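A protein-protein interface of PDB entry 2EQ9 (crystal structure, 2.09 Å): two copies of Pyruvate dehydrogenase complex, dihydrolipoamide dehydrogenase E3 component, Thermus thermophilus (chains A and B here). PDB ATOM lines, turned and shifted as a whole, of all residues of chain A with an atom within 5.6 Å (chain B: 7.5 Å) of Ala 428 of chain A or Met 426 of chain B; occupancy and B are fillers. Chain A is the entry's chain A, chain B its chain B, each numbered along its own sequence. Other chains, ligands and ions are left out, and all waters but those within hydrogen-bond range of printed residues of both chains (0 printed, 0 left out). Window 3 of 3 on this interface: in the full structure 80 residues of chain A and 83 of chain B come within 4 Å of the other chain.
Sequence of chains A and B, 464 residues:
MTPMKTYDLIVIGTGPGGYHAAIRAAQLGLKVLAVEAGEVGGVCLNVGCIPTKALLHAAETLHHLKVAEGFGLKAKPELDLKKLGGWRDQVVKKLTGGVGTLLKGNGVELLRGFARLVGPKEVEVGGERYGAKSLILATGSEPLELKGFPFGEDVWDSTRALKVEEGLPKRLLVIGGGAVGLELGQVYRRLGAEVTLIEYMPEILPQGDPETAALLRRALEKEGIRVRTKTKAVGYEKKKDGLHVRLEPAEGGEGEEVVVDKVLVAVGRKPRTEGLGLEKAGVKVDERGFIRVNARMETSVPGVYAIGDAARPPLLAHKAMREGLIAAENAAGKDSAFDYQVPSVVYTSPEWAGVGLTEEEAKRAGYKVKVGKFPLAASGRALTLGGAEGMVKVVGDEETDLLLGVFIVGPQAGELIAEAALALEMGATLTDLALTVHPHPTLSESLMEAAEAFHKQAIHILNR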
ATOM      1  N   ASP A 401      -3.460   0.335  -7.569  1.00  0.00           N
ATOM      2  CA  ASP A 401      -4.048   1.428  -6.785  1.00  0.00           C
ATOM      3  C   ASP A 401      -3.976   2.758  -7.554  1.00  0.00           C
ATOM      4  O   ASP A 401      -4.252   3.828  -7.010  1.00  0.00           O
ATOM      5  CB  ASP A 401      -3.324   1.572  -5.442  1.00  0.00           C
ATOM      6  CG  ASP A 401      -4.150   2.317  -4.412  1.00  0.00           C
ATOM      7  OD1 ASP A 401      -5.274   1.865  -4.112  1.00  0.00           O
ATOM      8  OD2 ASP A 401      -3.682   3.353  -3.897  1.00  0.00           O
ATOM      9  N   LEU A 402      -3.614   2.676  -8.823  1.00  0.00           N
ATOM     10  CA  LEU A 402      -3.482   3.859  -9.666  1.00  0.00           C
ATOM     11  C   LEU A 402      -4.835   4.419 -10.101  1.00  0.00           C
ATOM     12  O   LEU A 402      -5.739   3.658 -10.462  1.00  0.00           O
ATOM     13  CB  LEU A 402      -2.668   3.505 -10.905  1.00  0.00           C
ATOM     14  CG  LEU A 402      -1.990   4.654 -11.636  1.00  0.00           C
ATOM     15  CD1 LEU A 402      -0.750   5.088 -10.846  1.00  0.00           C
ATOM     16  CD2 LEU A 402      -1.614   4.194 -13.042  1.00  0.00           C
ATOM     17  N   LEU A 403      -4.967   5.746 -10.060  1.00  0.00           N
ATOM     18  CA  LEU A 403      -6.208   6.416 -10.469  1.00  0.00           C
ATOM     19  C   LEU A 403      -6.256   6.409 -11.988  1.00  0.00           C
ATOM     20  O   LEU A 403      -5.267   6.730 -12.648  1.00  0.00           O
ATOM     21  CB  LEU A 403      -6.238   7.864  -9.957  1.00  0.00           C
ATOM     22  CG  LEU A 403      -7.463   8.734 -10.291  1.00  0.00           C
ATOM     23  CD1 LEU A 403      -8.700   8.224  -9.566  1.00  0.00           C
ATOM     24  CD2 LEU A 403      -7.181  10.179  -9.852  1.00  0.00           C
ATOM     25  N   ALA A 423      -4.185  15.111 -10.486  1.00  0.00           N
ATOM     26  CA  ALA A 423      -3.932  13.807  -9.892  1.00  0.00           C
ATOM     27  C   ALA A 423      -3.447  12.850 -10.981  1.00  0.00           C
ATOM     28  O   ALA A 423      -2.443  12.162 -10.817  1.00  0.00           O
ATOM     29  CB  ALA A 423      -5.213  13.275  -9.228  1.00  0.00           C
ATOM     30  N   LEU A 424      -4.153  12.827 -12.101  1.00  0.00           N
ATOM     31  CA  LEU A 424      -3.785  11.963 -13.216  1.00  0.00           C
ATOM     32  C   LEU A 424      -2.410  12.321 -13.780  1.00  0.00           C
ATOM     33  O   LEU A 424      -1.571  11.443 -13.989  1.00  0.00           O
ATOM     34  CB  LEU A 424      -4.839  12.067 -14.326  1.00  0.00           C
ATOM     35  CG  LEU A 424      -6.233  11.527 -13.977  1.00  0.00           C
ATOM     36  CD1 LEU A 424      -7.202  11.795 -15.132  1.00  0.00           C
ATOM     37  CD2 LEU A 424      -6.137  10.024 -13.677  1.00  0.00           C
ATOM     38  N   MET A 426       0.043  13.631 -12.369  1.00  0.00           N
ATOM     39  CA  MET A 426       1.088  13.296 -11.402  1.00  0.00           C
ATOM     40  C   MET A 426       1.199  11.798 -11.096  1.00  0.00           C
ATOM     41  O   MET A 426       2.020  11.403 -10.269  1.00  0.00           O
ATOM     42  CB  MET A 426       0.853  14.044 -10.075  1.00  0.00           C
ATOM     43  CG  MET A 426       0.919  15.565 -10.153  1.00  0.00           C
ATOM     44  SD  MET A 426       2.518  16.238 -10.667  1.00  0.00           S
ATOM     45  CE  MET A 426       3.446  16.088  -9.172  1.00  0.00           C
ATOM     46  N   GLY A 427       0.376  10.978 -11.749  1.00  0.00           N
ATOM     47  CA  GLY A 427       0.406   9.539 -11.518  1.00  0.00           C
ATOM     48  C   GLY A 427      -0.067   9.146 -10.129  1.00  0.00           C
ATOM     49  O   GLY A 427       0.407   8.169  -9.540  1.00  0.00           O
ATOM     50  N   ALA A 428      -1.013   9.908  -9.598  1.00  0.00           N
ATOM     51  CA  ALA A 428      -1.538   9.654  -8.264  1.00  0.00           C
ATOM     52  C   ALA A 428      -2.264   8.323  -8.125  1.00  0.00           C
ATOM     53  O   ALA A 428      -2.815   7.802  -9.088  1.00  0.00           O
ATOM     54  CB  ALA A 428      -2.477  10.778  -7.865  1.00  0.00           C
ATOM     55  N   THR A 429      -2.253   7.779  -6.913  1.00  0.00           N
ATOM     56  CA  THR A 429      -2.949   6.532  -6.619  1.00  0.00           C
ATOM     57  C   THR A 429      -4.194   6.958  -5.856  1.00  0.00           C
ATOM     58  O   THR A 429      -4.305   8.118  -5.454  1.00  0.00           O
ATOM     59  CB  THR A 429      -2.125   5.629  -5.689  1.00  0.00           C
ATOM     60  OG1 THR A 429      -1.843   6.339  -4.479  1.00  0.00           O
ATOM     61  CG2 THR A 429      -0.814   5.208  -6.350  1.00  0.00           C
ATOM     62  N   LEU A 430      -5.126   6.037  -5.640  1.00  0.00           N
ATOM     63  CA  LEU A 430      -6.330   6.368  -4.890  1.00  0.00           C
ATOM     64  C   LEU A 430      -5.956   6.722  -3.452  1.00  0.00           C
ATOM     65  O   LEU A 430      -6.673   7.464  -2.779  1.00  0.00           O
ATOM     66  CB  LEU A 430      -7.315   5.193  -4.899  1.00  0.00           C
ATOM     67  CG  LEU A 430      -8.259   5.087  -6.098  1.00  0.00           C
ATOM     68  CD1 LEU A 430      -9.232   6.276  -6.070  1.00  0.00           C
ATOM     69  CD2 LEU A 430      -7.461   5.066  -7.396  1.00  0.00           C
ATOM     70  N   ASP A 432      -3.173   8.404  -2.526  1.00  0.00           N
ATOM     71  CA  ASP A 432      -2.660   9.773  -2.492  1.00  0.00           C
ATOM     72  C   ASP A 432      -3.854  10.725  -2.428  1.00  0.00           C
ATOM     73  O   ASP A 432      -3.845  11.717  -1.698  1.00  0.00           O
ATOM     74  CB  ASP A 432      -1.840  10.090  -3.752  1.00  0.00           C
ATOM     75  CG  ASP A 432      -0.534   9.305  -3.824  1.00  0.00           C
ATOM     76  OD1 ASP A 432       0.097   9.108  -2.764  1.00  0.00           O
ATOM     77  OD2 ASP A 432      -0.134   8.897  -4.942  1.00  0.00           O
ATOM     78  N   LEU A 433      -4.887  10.408  -3.202  1.00  0.00           N
ATOM     79  CA  LEU A 433      -6.093  11.225  -3.240  1.00  0.00           C
ATOM     80  C   LEU A 433      -6.710  11.249  -1.841  1.00  0.00           C
ATOM     81  O   LEU A 433      -7.095  12.305  -1.331  1.00  0.00           O
ATOM     82  CB  LEU A 433      -7.071  10.629  -4.251  1.00  0.00           C
ATOM     83  CG  LEU A 433      -8.061  11.561  -4.947  1.00  0.00           C
ATOM     84  CD1 LEU A 433      -7.328  12.795  -5.486  1.00  0.00           C
ATOM     85  CD2 LEU A 433      -8.736  10.808  -6.095  1.00  0.00           C
ATOM     86  N   LEU B 402      10.058  23.833  -7.160  1.00  0.00           N
ATOM     87  CA  LEU B 402       9.092  23.183  -6.279  1.00  0.00           C
ATOM     88  C   LEU B 402       8.047  24.132  -5.696  1.00  0.00           C
ATOM     89  O   LEU B 402       8.386  25.193  -5.172  1.00  0.00           O
ATOM     90  CB  LEU B 402       9.822  22.479  -5.131  1.00  0.00           C
ATOM     91  CG  LEU B 402       9.000  21.584  -4.201  1.00  0.00           C
ATOM     92  CD1 LEU B 402       8.574  20.319  -4.945  1.00  0.00           C
ATOM     93  CD2 LEU B 402       9.830  21.210  -2.979  1.00  0.00           C
ATOM     94  N   GLU B 419      -6.833  21.375  -4.687  1.00  0.00           N
ATOM     95  CA  GLU B 419      -5.940  21.033  -5.781  1.00  0.00           C
ATOM     96  C   GLU B 419      -4.516  21.403  -5.378  1.00  0.00           C
ATOM     97  O   GLU B 419      -3.557  20.688  -5.686  1.00  0.00           O
ATOM     98  CB  GLU B 419      -6.307  21.814  -7.036  1.00  0.00           C
ATOM     99  CG  GLU B 419      -5.418  21.475  -8.220  1.00  0.00           C
ATOM    100  CD  GLU B 419      -5.601  22.419  -9.387  1.00  0.00           C
ATOM    101  OE1 GLU B 419      -6.662  23.075  -9.467  1.00  0.00           O
ATOM    102  OE2 GLU B 419      -4.686  22.493 -10.236  1.00  0.00           O
ATOM    103  N   ALA B 420      -4.388  22.538  -4.697  1.00  0.00           N
ATOM    104  CA  ALA B 420      -3.084  23.015  -4.255  1.00  0.00           C
ATOM    105  C   ALA B 420      -2.534  22.044  -3.223  1.00  0.00           C
ATOM    106  O   ALA B 420      -1.354  21.707  -3.251  1.00  0.00           O
ATOM    107  CB  ALA B 420      -3.204  24.423  -3.657  1.00  0.00           C
ATOM    108  N   ALA B 421      -3.401  21.600  -2.315  1.00  0.00           N
ATOM    109  CA  ALA B 421      -3.005  20.650  -1.284  1.00  0.00           C
ATOM    110  C   ALA B 421      -2.517  19.347  -1.930  1.00  0.00           C
ATOM    111  O   ALA B 421      -1.470  18.819  -1.547  1.00  0.00           O
ATOM    112  CB  ALA B 421      -4.172  20.373  -0.335  1.00  0.00           C
ATOM    113  N   LEU B 422      -3.268  18.828  -2.900  1.00  0.00           N
ATOM    114  CA  LEU B 422      -2.852  17.599  -3.584  1.00  0.00           C
ATOM    115  C   LEU B 422      -1.500  17.871  -4.220  1.00  0.00           C
ATOM    116  O   LEU B 422      -0.574  17.070  -4.103  1.00  0.00           O
ATOM    117  CB  LEU B 422      -3.849  17.201  -4.676  1.00  0.00           C
ATOM    118  CG  LEU B 422      -3.422  15.990  -5.527  1.00  0.00           C
ATOM    119  CD1 LEU B 422      -3.383  14.732  -4.649  1.00  0.00           C
ATOM    120  CD2 LEU B 422      -4.386  15.791  -6.692  1.00  0.00           C
ATOM    121  N   ALA B 423      -1.388  19.011  -4.896  1.00  0.00           N
ATOM    122  CA  ALA B 423      -0.128  19.383  -5.535  1.00  0.00           C
ATOM    123  C   ALA B 423       1.034  19.275  -4.547  1.00  0.00           C
ATOM    124  O   ALA B 423       2.043  18.650  -4.845  1.00  0.00           O
ATOM    125  CB  ALA B 423      -0.210  20.803  -6.086  1.00  0.00           C
ATOM    126  N   LEU B 424       0.883  19.868  -3.365  1.00  0.00           N
ATOM    127  CA  LEU B 424       1.951  19.827  -2.375  1.00  0.00           C
ATOM    128  C   LEU B 424       2.275  18.391  -1.961  1.00  0.00           C
ATOM    129  O   LEU B 424       3.441  18.008  -1.921  1.00  0.00           O
ATOM    130  CB  LEU B 424       1.583  20.680  -1.147  1.00  0.00           C
ATOM    131  CG  LEU B 424       1.466  22.199  -1.407  1.00  0.00           C
ATOM    132  CD1 LEU B 424       0.990  22.917  -0.142  1.00  0.00           C
ATOM    133  CD2 LEU B 424       2.822  22.758  -1.851  1.00  0.00           C
ATOM    134  N   GLU B 425       1.244  17.603  -1.666  1.00  0.00           N
ATOM    135  CA  GLU B 425       1.428  16.215  -1.265  1.00  0.00           C
ATOM    136  C   GLU B 425       2.149  15.409  -2.344  1.00  0.00           C
ATOM    137  O   GLU B 425       2.991  14.571  -2.029  1.00  0.00           O
ATOM    138  CB  GLU B 425       0.076  15.558  -0.962  1.00  0.00           C
ATOM    139  CG  GLU B 425      -0.667  16.118   0.247  1.00  0.00           C
ATOM    140  CD  GLU B 425       0.163  16.099   1.525  1.00  0.00           C
ATOM    141  OE1 GLU B 425       1.046  15.222   1.656  1.00  0.00           O
ATOM    142  OE2 GLU B 425      -0.083  16.956   2.406  1.00  0.00           O
ATOM    143  N   MET B 426       1.828  15.669  -3.611  1.00  0.00           N
ATOM    144  CA  MET B 426       2.462  14.957  -4.724  1.00  0.00           C
ATOM    145  C   MET B 426       3.833  15.535  -5.102  1.00  0.00           C
ATOM    146  O   MET B 426       4.485  15.040  -6.023  1.00  0.00           O
ATOM    147  CB  MET B 426       1.566  14.995  -5.968  1.00  0.00           C
ATOM    148  CG  MET B 426       0.191  14.368  -5.800  1.00  0.00           C
ATOM    149  SD  MET B 426       0.270  12.635  -5.383  1.00  0.00           S
ATOM    150  CE  MET B 426       0.983  11.952  -6.885  1.00  0.00           C
ATOM    151  N   GLY B 427       4.265  16.584  -4.408  1.00  0.00           N
ATOM    152  CA  GLY B 427       5.555  17.185  -4.723  1.00  0.00           C
ATOM    153  C   GLY B 427       5.588  17.806  -6.110  1.00  0.00           C
ATOM    154  O   GLY B 427       6.574  17.704  -6.843  1.00  0.00           O
ATOM    155  N   ALA B 428       4.498  18.463  -6.481  1.00  0.00           N
ATOM    156  CA  ALA B 428       4.426  19.086  -7.789  1.00  0.00           C
ATOM    157  C   ALA B 428       5.298  20.347  -7.877  1.00  0.00           C
ATOM    158  O   ALA B 428       5.494  21.048  -6.884  1.00  0.00           O
ATOM    159  CB  ALA B 428       2.977  19.436  -8.101  1.00  0.00           C
ATOM    160  N   THR B 429       5.827  20.604  -9.071  1.00  0.00           N
ATOM    161  CA  THR B 429       6.619  21.798  -9.344  1.00  0.00           C
ATOM    162  C   THR B 429       5.649  22.811  -9.966  1.00  0.00           C
ATOM    163  O   THR B 429       4.497  22.460 -10.280  1.00  0.00           O
ATOM    164  CB  THR B 429       7.721  21.519 -10.375  1.00  0.00           C
ATOM    165  OG1 THR B 429       7.123  20.985 -11.562  1.00  0.00           O
ATOM    166  CG2 THR B 429       8.761  20.530  -9.813  1.00  0.00           C
ATOM    167  N   ASP B 432       4.551  21.565 -13.273  1.00  0.00           N
ATOM    168  CA  ASP B 432       3.536  20.515 -13.241  1.00  0.00           C
ATOM    169  C   ASP B 432       2.158  21.154 -13.150  1.00  0.00           C
ATOM    170  O   ASP B 432       1.220  20.728 -13.816  1.00  0.00           O
ATOM    171  CB  ASP B 432       3.721  19.581 -12.040  1.00  0.00           C
ATOM    172  CG  ASP B 432       4.993  18.761 -12.119  1.00  0.00           C
ATOM    173  OD1 ASP B 432       5.311  18.243 -13.210  1.00  0.00           O
ATOM    174  OD2 ASP B 432       5.664  18.615 -11.079  1.00  0.00           O
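Among the printed residues, merely in contact across the chains: Met 426 of chain A with Ala 428 of chain B (3.4 Å), Met 426 of chain A with Met 426 of chain B (3.5 Å), Ala 423 of chain A with Leu 422 of chain B (3.7 Å), Ala 428 of chain A with Met 426 of chain B (3.7 Å) and Met 426 of chain A with Asp 432 of chain B (3.8 Å).
The side-chain carboxylate of Asp 432 of chain A lies close to the side-chain sulfur of Met 426 of chain B, at 3.8 Å.
Of the 13 printed residues of chain B, 4 touch a printed residue of chain A.
Printed residues of chain B that touch a printed residue of chain A: Leu 422, Met 426, Ala 428 and Asp 432.
Along chain B the printed residues that touch a printed residue of chain A span positions 422 to 432.
Among the printed residues, 6 pairs touch across the chains.
Met 426 of chain A touches its own counterpart, Met 426 of chain B.
Met 426 of chain A touches Ala 428 of chain B, and with the chains exchanged Ala 428 of chain A touches Met 426 of chain B.
Met 426 of chain A touches Asp 432 of chain B, and with the chains exchanged Asp 432 of chain A touches Met 426 of chain B.
The backbone carbonyl oxygen (O) of Ala 428 of chain A lies within hydrogen-bond range of the backbone NH (N) of Leu 403 of chain A (3.1 Å).
The backbone carbonyl oxygen (O) of Ala 423 of chain A sits at hydrogen-bond distance from the backbone NH (N) of Ala 428 of chain A (2.9 Å).
The side-chain carboxylate (OD2) of Asp 432 of chain A sits at hydrogen-bond distance from the backbone NH (N) of Thr 429 of chain A (3.1 Å).
N of Ala 428 of chain B sits at hydrogen-bond distance from O of Ala 423 of chain B (3.0 Å).
OG1 of Thr 429 of chain B lies within hydrogen-bond range of OD2 of Asp 432 of chain B (2.8 Å).
Of chain B, only Met 426 (3.7 Å) comes within 4 Å of Ala 428 of chain A.
Met 426 of chain B touches just these residues of chain A: Met 426, Ala 428 and Asp 432.
No residue of chain B comes within 4 Å of Gly 427 of chain A.
Printed residues of chain B within 4 Å of Met 426 of chain A: Met 426 (3.5 Å), Ala 428 (3.4 Å) and Asp 432 (3.8 Å).
Of the printed residues of chain B, Ala 423 of chain A touches Leu 422.
Printed residues of chain A within 4 Å of Leu 422 of chain B: Ala 423 (3.7 Å).
Asp 401 of chain A touches none of the printed residues of chain B.
Ala 421 of chain B touches none of the printed residues of chain A.
The nearest residue of chain B that does not touch Ala 428 of chain A is Leu 422 of chain B (5.2 Å).
The nearest printed residue of chain B that does not touch Asp 432 of chain A is Leu 422 of chain B (4.2 Å).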
